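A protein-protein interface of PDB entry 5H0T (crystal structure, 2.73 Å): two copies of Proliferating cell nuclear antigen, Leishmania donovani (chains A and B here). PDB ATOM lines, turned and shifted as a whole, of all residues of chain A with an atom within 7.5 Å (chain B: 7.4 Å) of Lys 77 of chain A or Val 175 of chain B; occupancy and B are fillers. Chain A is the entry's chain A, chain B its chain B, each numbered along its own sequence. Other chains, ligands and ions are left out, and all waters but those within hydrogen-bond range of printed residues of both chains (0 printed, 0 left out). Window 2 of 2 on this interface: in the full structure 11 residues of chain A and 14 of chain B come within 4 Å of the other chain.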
ATOM      1  N   VAL A  16       4.843 -10.605   5.816  1.00  0.00           N
ATOM      2  CA  VAL A  16       3.849 -11.627   6.026  1.00  0.00           C
ATOM      3  C   VAL A  16       3.141 -11.479   7.353  1.00  0.00           C
ATOM      4  O   VAL A  16       1.937 -11.640   7.406  1.00  0.00           O
ATOM      5  CB  VAL A  16       4.419 -13.017   5.848  1.00  0.00           C
ATOM      6  CG1 VAL A  16       3.358 -14.022   6.173  1.00  0.00           C
ATOM      7  CG2 VAL A  16       4.830 -13.202   4.382  1.00  0.00           C
ATOM      8  N   GLU A  17       3.872 -11.149   8.411  1.00  0.00           N
ATOM      9  CA  GLU A  17       3.246 -10.784   9.682  1.00  0.00           C
ATOM     10  C   GLU A  17       2.190  -9.729   9.495  1.00  0.00           C
ATOM     11  O   GLU A  17       1.074  -9.874   9.994  1.00  0.00           O
ATOM     12  CB  GLU A  17       4.278 -10.296  10.690  1.00  0.00           C
ATOM     13  CG  GLU A  17       5.174 -11.418  11.244  1.00  0.00           C
ATOM     14  CD  GLU A  17       4.375 -12.383  12.119  1.00  0.00           C
ATOM     15  OE1 GLU A  17       3.812 -11.844  13.126  1.00  0.00           O
ATOM     16  OE2 GLU A  17       4.341 -13.616  11.851  1.00  0.00           O
ATOM     17  N   ASN A  20      -0.801 -11.172   7.151  1.00  0.00           N
ATOM     18  CA  ASN A  20      -1.451 -12.287   7.843  1.00  0.00           C
ATOM     19  C   ASN A  20      -2.350 -11.838   9.009  1.00  0.00           C
ATOM     20  O   ASN A  20      -3.321 -12.521   9.386  1.00  0.00           O
ATOM     21  CB  ASN A  20      -0.417 -13.224   8.407  1.00  0.00           C
ATOM     22  CG  ASN A  20      -0.980 -14.547   8.834  1.00  0.00           C
ATOM     23  OD1 ASN A  20      -2.069 -14.970   8.410  1.00  0.00           O
ATOM     24  ND2 ASN A  20      -0.192 -15.242   9.622  1.00  0.00           N
ATOM     25  N   ASN A  71      -1.410 -19.956   1.634  1.00  0.00           N
ATOM     26  CA  ASN A  71      -1.785 -19.914   3.008  1.00  0.00           C
ATOM     27  C   ASN A  71      -0.767 -19.079   3.782  1.00  0.00           C
ATOM     28  O   ASN A  71       0.360 -19.489   3.989  1.00  0.00           O
ATOM     29  CB  ASN A  71      -1.833 -21.321   3.579  1.00  0.00           C
ATOM     30  CG  ASN A  71      -2.602 -21.391   4.857  1.00  0.00           C
ATOM     31  OD1 ASN A  71      -2.613 -20.474   5.666  1.00  0.00           O
ATOM     32  ND2 ASN A  71      -3.294 -22.461   5.025  1.00  0.00           N
ATOM     33  N   LEU A  72      -1.189 -17.915   4.238  1.00  0.00           N
ATOM     34  CA  LEU A  72      -0.316 -17.003   4.943  1.00  0.00           C
ATOM     35  C   LEU A  72      -0.019 -17.479   6.340  1.00  0.00           C
ATOM     36  O   LEU A  72       1.018 -17.149   6.893  1.00  0.00           O
ATOM     37  CB  LEU A  72      -0.935 -15.627   5.016  1.00  0.00           C
ATOM     38  CG  LEU A  72      -1.139 -15.019   3.614  1.00  0.00           C
ATOM     39  CD1 LEU A  72      -1.889 -13.738   3.768  1.00  0.00           C
ATOM     40  CD2 LEU A  72       0.167 -14.762   2.926  1.00  0.00           C
ATOM     41  N   ALA A  73      -0.943 -18.249   6.926  1.00  0.00           N
ATOM     42  CA  ALA A  73      -0.692 -18.912   8.188  1.00  0.00           C
ATOM     43  C   ALA A  73       0.503 -19.863   8.063  1.00  0.00           C
ATOM     44  O   ALA A  73       1.461 -19.733   8.810  1.00  0.00           O
ATOM     45  CB  ALA A  73      -1.933 -19.613   8.654  1.00  0.00           C
ATOM     46  N   SER A  74       0.481 -20.777   7.090  1.00  0.00           N
ATOM     47  CA  SER A  74       1.656 -21.633   6.848  1.00  0.00           C
ATOM     48  C   SER A  74       2.894 -20.851   6.488  1.00  0.00           C
ATOM     49  O   SER A  74       3.983 -21.161   6.966  1.00  0.00           O
ATOM     50  CB  SER A  74       1.409 -22.617   5.727  1.00  0.00           C
ATOM     51  OG  SER A  74       0.193 -23.300   5.933  1.00  0.00           O
ATOM     52  N   LEU A  75       2.751 -19.872   5.605  1.00  0.00           N
ATOM     53  CA  LEU A  75       3.886 -19.096   5.165  1.00  0.00           C
ATOM     54  C   LEU A  75       4.513 -18.405   6.379  1.00  0.00           C
ATOM     55  O   LEU A  75       5.717 -18.404   6.529  1.00  0.00           O
ATOM     56  CB  LEU A  75       3.471 -18.072   4.111  1.00  0.00           C
ATOM     57  CG  LEU A  75       4.554 -17.198   3.493  1.00  0.00           C
ATOM     58  CD1 LEU A  75       5.575 -18.054   2.806  1.00  0.00           C
ATOM     59  CD2 LEU A  75       3.911 -16.201   2.493  1.00  0.00           C
ATOM     60  N   SER A  76       3.671 -17.876   7.260  1.00  0.00           N
ATOM     61  CA  SER A  76       4.127 -17.199   8.466  1.00  0.00           C
ATOM     62  C   SER A  76       4.945 -18.137   9.335  1.00  0.00           C
ATOM     63  O   SER A  76       6.002 -17.754   9.824  1.00  0.00           O
ATOM     64  CB  SER A  76       2.952 -16.614   9.281  1.00  0.00           C
ATOM     65  OG  SER A  76       3.382 -15.481  10.026  1.00  0.00           O
ATOM     66  N   LYS A  77       4.466 -19.375   9.484  1.00  0.00           N
ATOM     67  CA  LYS A  77       5.145 -20.399  10.272  1.00  0.00           C
ATOM     68  C   LYS A  77       6.500 -20.776   9.733  1.00  0.00           C
ATOM     69  O   LYS A  77       7.443 -21.012  10.511  1.00  0.00           O
ATOM     70  CB  LYS A  77       4.293 -21.637  10.379  1.00  0.00           C
ATOM     71  CG  LYS A  77       3.085 -21.402  11.274  1.00  0.00           C
ATOM     72  CD  LYS A  77       2.127 -22.586  11.286  1.00  0.00           C
ATOM     73  CE  LYS A  77       0.766 -22.175  11.816  1.00  0.00           C
ATOM     74  NZ  LYS A  77      -0.259 -23.059  11.204  1.00  0.00           N
ATOM     75  N   VAL A  78       6.620 -20.822   8.416  1.00  0.00           N
ATOM     76  CA  VAL A  78       7.905 -21.121   7.826  1.00  0.00           C
ATOM     77  C   VAL A  78       8.812 -19.921   7.967  1.00  0.00           C
ATOM     78  O   VAL A  78       9.973 -20.049   8.286  1.00  0.00           O
ATOM     79  CB  VAL A  78       7.733 -21.536   6.352  1.00  0.00           C
ATOM     80  CG1 VAL A  78       9.067 -21.684   5.651  1.00  0.00           C
ATOM     81  CG2 VAL A  78       6.963 -22.821   6.305  1.00  0.00           C
ATOM     82  N   LEU A  79       8.289 -18.733   7.733  1.00  0.00           N
ATOM     83  CA  LEU A  79       9.141 -17.567   7.799  1.00  0.00           C
ATOM     84  C   LEU A  79       9.629 -17.313   9.211  1.00  0.00           C
ATOM     85  O   LEU A  79      10.759 -16.878   9.344  1.00  0.00           O
ATOM     86  CB  LEU A  79       8.473 -16.333   7.208  1.00  0.00           C
ATOM     87  CG  LEU A  79       8.183 -16.417   5.722  1.00  0.00           C
ATOM     88  CD1 LEU A  79       7.310 -15.266   5.298  1.00  0.00           C
ATOM     89  CD2 LEU A  79       9.424 -16.399   4.938  1.00  0.00           C
ATOM     90  N   LYS A  80       8.817 -17.605  10.242  1.00  0.00           N
ATOM     91  CA  LYS A  80       9.282 -17.536  11.659  1.00  0.00           C
ATOM     92  C   LYS A  80      10.612 -18.237  11.854  1.00  0.00           C
ATOM     93  O   LYS A  80      11.425 -17.757  12.601  1.00  0.00           O
ATOM     94  CB  LYS A  80       8.305 -18.083  12.669  1.00  0.00           C
ATOM     95  CG  LYS A  80       7.594 -16.890  13.297  1.00  0.00           C
ATOM     96  CD  LYS A  80       6.534 -17.408  14.193  1.00  0.00           C
ATOM     97  CE  LYS A  80       5.117 -16.786  14.012  1.00  0.00           C
ATOM     98  NZ  LYS A  80       4.095 -17.813  13.588  1.00  0.00           N
ATOM     99  N   ILE A  81      10.821 -19.344  11.173  1.00  0.00           N
ATOM    100  CA  ILE A  81      12.070 -20.055  11.332  1.00  0.00           C
ATOM    101  C   ILE A  81      13.186 -19.679  10.384  1.00  0.00           C
ATOM    102  O   ILE A  81      14.200 -20.300  10.425  1.00  0.00           O
ATOM    103  CB  ILE A  81      11.870 -21.583  11.248  1.00  0.00           C
ATOM    104  CG1 ILE A  81      11.784 -22.058   9.800  1.00  0.00           C
ATOM    105  CG2 ILE A  81      10.706 -22.016  12.142  1.00  0.00           C
ATOM    106  CD1 ILE A  81      11.132 -23.413   9.661  1.00  0.00           C
ATOM    107  N   VAL A  82      13.017 -18.708   9.519  1.00  0.00           N
ATOM    108  CA  VAL A  82      14.110 -18.324   8.613  1.00  0.00           C
ATOM    109  C   VAL A  82      14.873 -17.196   9.271  1.00  0.00           C
ATOM    110  O   VAL A  82      14.270 -16.242   9.749  1.00  0.00           O
ATOM    111  CB  VAL A  82      13.588 -17.869   7.246  1.00  0.00           C
ATOM    112  CG1 VAL A  82      14.738 -17.418   6.365  1.00  0.00           C
ATOM    113  CG2 VAL A  82      12.848 -19.009   6.581  1.00  0.00           C
ATOM    114  N   GLN A 115       8.760 -26.033   1.097  1.00  0.00           N
ATOM    115  CA  GLN A 115       7.789 -26.111   0.011  1.00  0.00           C
ATOM    116  C   GLN A 115       6.385 -25.969   0.512  1.00  0.00           C
ATOM    117  O   GLN A 115       5.965 -26.742   1.392  1.00  0.00           O
ATOM    118  CB  GLN A 115       7.836 -27.472  -0.614  1.00  0.00           C
ATOM    119  CG  GLN A 115       9.203 -27.855  -1.106  1.00  0.00           C
ATOM    120  CD  GLN A 115       9.144 -28.926  -2.157  1.00  0.00           C
ATOM    121  OE1 GLN A 115      10.050 -29.018  -2.981  1.00  0.00           O
ATOM    122  NE2 GLN A 115       8.048 -29.706  -2.181  1.00  0.00           N
ATOM    123  N   LEU A 116       5.632 -25.026  -0.054  1.00  0.00           N
ATOM    124  CA  LEU A 116       4.250 -24.823   0.347  1.00  0.00           C
ATOM    125  C   LEU A 116       3.324 -25.215  -0.791  1.00  0.00           C
ATOM    126  O   LEU A 116       3.644 -24.985  -1.960  1.00  0.00           O
ATOM    127  CB  LEU A 116       4.049 -23.363   0.748  1.00  0.00           C
ATOM    128  CG  LEU A 116       4.527 -22.866   2.110  1.00  0.00           C
ATOM    129  CD1 LEU A 116       5.593 -23.735   2.674  1.00  0.00           C
ATOM    130  CD2 LEU A 116       5.098 -21.453   2.015  1.00  0.00           C
ATOM    131  N   LYS A 117       2.195 -25.819  -0.448  1.00  0.00           N
ATOM    132  CA  LYS A 117       1.230 -26.221  -1.474  1.00  0.00           C
ATOM    133  C   LYS A 117       0.474 -24.996  -1.842  1.00  0.00           C
ATOM    134  O   LYS A 117       0.206 -24.202  -0.961  1.00  0.00           O
ATOM    135  CB  LYS A 117       0.255 -27.335  -1.015  1.00  0.00           C
ATOM    136  CG  LYS A 117       0.825 -28.712  -0.879  1.00  0.00           C
ATOM    137  CD  LYS A 117       0.488 -29.835  -1.931  1.00  0.00           C
ATOM    138  CE  LYS A 117       1.409 -31.016  -1.673  1.00  0.00           C
ATOM    139  NZ  LYS A 117       2.055 -31.638  -2.883  1.00  0.00           N
ATOM    140  N   ASP B 150      12.927 -25.876  14.389  1.00  0.00           N
ATOM    141  CA  ASP B 150      12.475 -25.564  13.065  1.00  0.00           C
ATOM    142  C   ASP B 150      11.738 -26.719  12.476  1.00  0.00           C
ATOM    143  O   ASP B 150      10.601 -26.558  12.072  1.00  0.00           O
ATOM    144  CB  ASP B 150      13.661 -25.190  12.141  1.00  0.00           C
ATOM    145  CG  ASP B 150      14.300 -23.816  12.481  1.00  0.00           C
ATOM    146  OD1 ASP B 150      13.854 -23.088  13.468  1.00  0.00           O
ATOM    147  OD2 ASP B 150      15.251 -23.480  11.705  1.00  0.00           O
ATOM    148  N   GLN B 152      10.218 -29.043  13.738  1.00  0.00           N
ATOM    149  CA  GLN B 152       8.924 -29.197  14.392  1.00  0.00           C
ATOM    150  C   GLN B 152       7.773 -28.389  13.813  1.00  0.00           C
ATOM    151  O   GLN B 152       6.641 -28.702  14.137  1.00  0.00           O
ATOM    152  CB  GLN B 152       9.038 -28.952  15.896  1.00  0.00           C
ATOM    153  CG  GLN B 152       9.785 -30.078  16.573  1.00  0.00           C
ATOM    154  CD  GLN B 152      10.158 -29.814  18.007  1.00  0.00           C
ATOM    155  OE1 GLN B 152      11.064 -29.014  18.307  1.00  0.00           O
ATOM    156  NE2 GLN B 152       9.489 -30.547  18.912  1.00  0.00           N
ATOM    157  N   VAL B 153       8.008 -27.378  12.962  1.00  0.00           N
ATOM    158  CA  VAL B 153       6.861 -26.673  12.359  1.00  0.00           C
ATOM    159  C   VAL B 153       6.185 -27.580  11.364  1.00  0.00           C
ATOM    160  O   VAL B 153       4.979 -27.428  11.129  1.00  0.00           O
ATOM    161  CB  VAL B 153       7.162 -25.281  11.715  1.00  0.00           C
ATOM    162  CG1 VAL B 153       8.097 -24.439  12.588  1.00  0.00           C
ATOM    163  CG2 VAL B 153       7.689 -25.415  10.301  1.00  0.00           C
ATOM    164  N   PHE B 154       6.948 -28.529  10.804  1.00  0.00           N
ATOM    165  CA  PHE B 154       6.420 -29.445   9.798  1.00  0.00           C
ATOM    166  C   PHE B 154       5.825 -30.681  10.406  1.00  0.00           C
ATOM    167  O   PHE B 154       4.643 -30.898  10.281  1.00  0.00           O
ATOM    168  CB  PHE B 154       7.478 -29.756   8.765  1.00  0.00           C
ATOM    169  CG  PHE B 154       7.991 -28.534   8.110  1.00  0.00           C
ATOM    170  CD1 PHE B 154       7.274 -27.914   7.096  1.00  0.00           C
ATOM    171  CD2 PHE B 154       9.123 -27.925   8.588  1.00  0.00           C
ATOM    172  CE1 PHE B 154       7.714 -26.746   6.536  1.00  0.00           C
ATOM    173  CE2 PHE B 154       9.585 -26.752   8.032  1.00  0.00           C
ATOM    174  CZ  PHE B 154       8.881 -26.166   6.994  1.00  0.00           C
ATOM    175  N   GLY B 155       6.633 -31.450  11.105  1.00  0.00           N
ATOM    176  CA  GLY B 155       6.239 -32.752  11.631  1.00  0.00           C
ATOM    177  C   GLY B 155       6.656 -33.066  13.043  1.00  0.00           C
ATOM    178  O   GLY B 155       7.161 -32.218  13.780  1.00  0.00           O
ATOM    179  N   SER B 172       8.167 -33.385   7.362  1.00  0.00           N
ATOM    180  CA  SER B 172       6.911 -33.172   6.582  1.00  0.00           C
ATOM    181  C   SER B 172       5.683 -33.083   7.434  1.00  0.00           C
ATOM    182  O   SER B 172       5.660 -33.542   8.563  1.00  0.00           O
ATOM    183  CB  SER B 172       6.673 -34.305   5.631  1.00  0.00           C
ATOM    184  OG  SER B 172       7.344 -34.022   4.450  1.00  0.00           O
ATOM    185  N   GLY B 173       4.634 -32.518   6.865  1.00  0.00           N
ATOM    186  CA  GLY B 173       3.407 -32.297   7.621  1.00  0.00           C
ATOM    187  C   GLY B 173       2.420 -31.437   6.894  1.00  0.00           C
ATOM    188  O   GLY B 173       2.543 -31.211   5.700  1.00  0.00           O
ATOM    189  N   ASP B 174       1.430 -30.958   7.645  1.00  0.00           N
ATOM    190  CA  ASP B 174       0.328 -30.173   7.100  1.00  0.00           C
ATOM    191  C   ASP B 174       0.893 -28.889   6.504  1.00  0.00           C
ATOM    192  O   ASP B 174       0.671 -28.609   5.335  1.00  0.00           O
ATOM    193  CB  ASP B 174      -0.694 -29.900   8.230  1.00  0.00           C
ATOM    194  CG  ASP B 174      -2.029 -29.397   7.756  1.00  0.00           C
ATOM    195  OD1 ASP B 174      -2.443 -29.765   6.641  1.00  0.00           O
ATOM    196  OD2 ASP B 174      -2.686 -28.659   8.539  1.00  0.00           O
ATOM    197  N   VAL B 175       1.676 -28.156   7.291  1.00  0.00           N
ATOM    198  CA  VAL B 175       2.295 -26.906   6.823  1.00  0.00           C
ATOM    199  C   VAL B 175       3.074 -27.076   5.492  1.00  0.00           C
ATOM    200  O   VAL B 175       3.014 -26.207   4.607  1.00  0.00           O
ATOM    201  CB  VAL B 175       3.168 -26.311   7.929  1.00  0.00           C
ATOM    202  CG1 VAL B 175       4.135 -25.273   7.412  1.00  0.00           C
ATOM    203  CG2 VAL B 175       2.296 -25.712   9.035  1.00  0.00           C
ATOM    204  N   GLY B 176       3.761 -28.202   5.336  1.00  0.00           N
ATOM    205  CA  GLY B 176       4.507 -28.473   4.123  1.00  0.00           C
ATOM    206  C   GLY B 176       5.674 -29.404   4.348  1.00  0.00           C
ATOM    207  O   GLY B 176       5.576 -30.343   5.135  1.00  0.00           O
ATOM    208  N   GLN B 177       6.772 -29.141   3.644  1.00  0.00           N
ATOM    209  CA  GLN B 177       7.990 -29.952   3.733  1.00  0.00           C
ATOM    210  C   GLN B 177       9.155 -29.028   3.917  1.00  0.00           C
ATOM    211  O   GLN B 177       9.224 -27.998   3.281  1.00  0.00           O
ATOM    212  CB  GLN B 177       8.224 -30.686   2.444  1.00  0.00           C
ATOM    213  CG  GLN B 177       7.081 -31.553   1.946  1.00  0.00           C
ATOM    214  CD  GLN B 177       7.291 -31.884   0.490  1.00  0.00           C
ATOM    215  OE1 GLN B 177       8.422 -32.151   0.114  1.00  0.00           O
ATOM    216  NE2 GLN B 177       6.235 -31.795  -0.347  1.00  0.00           N
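Lys 77 of chain A touches Val 175 of chain B. Val 78 of chain A touches Phe 154 of chain B. CG1 of Val 175 of chain B touches CG2 of Val 78 of chain A, at 3.9 Å. Ile 81 of chain A touches Asp 150 of chain B (CB to OD1, 3.3 Å). Ile 81 of chain A touches Val 153 of chain B (CG2 to CG1, 3.6 Å). CA of Gly 176 of chain B touches O of Gln 115 of chain A (3.5 Å).
Lys 77 of chain A touches just one residue of chain B: Val 175. Val 175 of chain B touches two residues of chain A. Printed residues of chain A within 4 Å of Phe 154 of chain B: Val 78. Printed residues of chain B within 4 Å of Val 78 of chain A: Phe 154 (3.9 Å) and Val 175 (3.9 Å). Printed residues of chain A within 4 Å of Val 153 of chain B: Ile 81. Of the printed residues of chain B, Gln 115 of chain A touches Gly 176 (3.5 Å) and Gln 177 (3.0 Å). Gly 173 of chain B touches none of the printed residues of chain A. The nearest printed residue of chain A that does not touch Val 175 of chain B is Leu 116 of chain A (4.1 Å). The nearest printed residue of chain A that does not touch Gln 177 of chain B is Lys 117 of chain A (4.9 Å).
Of the 11 printed residues of chain B, 6 touch a printed residue of chain A. Printed residues of chain B that touch a printed residue of chain A: Asp 150, Val 153, Phe 154, Val 175, Gly 176 and Gln 177. Hydrophobic or aromatic side chains of chain B within 4 Å of the printed part of chain A: Val 153, Phe 154 and Val 175. Among the printed residues, 7 pairs touch across the chains. Among the printed residues, no Asp or Glu carboxylate lies within 4 Å of a Lys or Arg side-chain nitrogen of the other chain.
No position is printed for both chains. Of the 7 pairs that touch across the chains among the printed residues, none has its exchanged pair printed and touching as well.
The backbone carbonyl oxygen of Gln 177 of chain B sits at hydrogen-bond distance from the backbone NH of Gln 115 of chain A.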
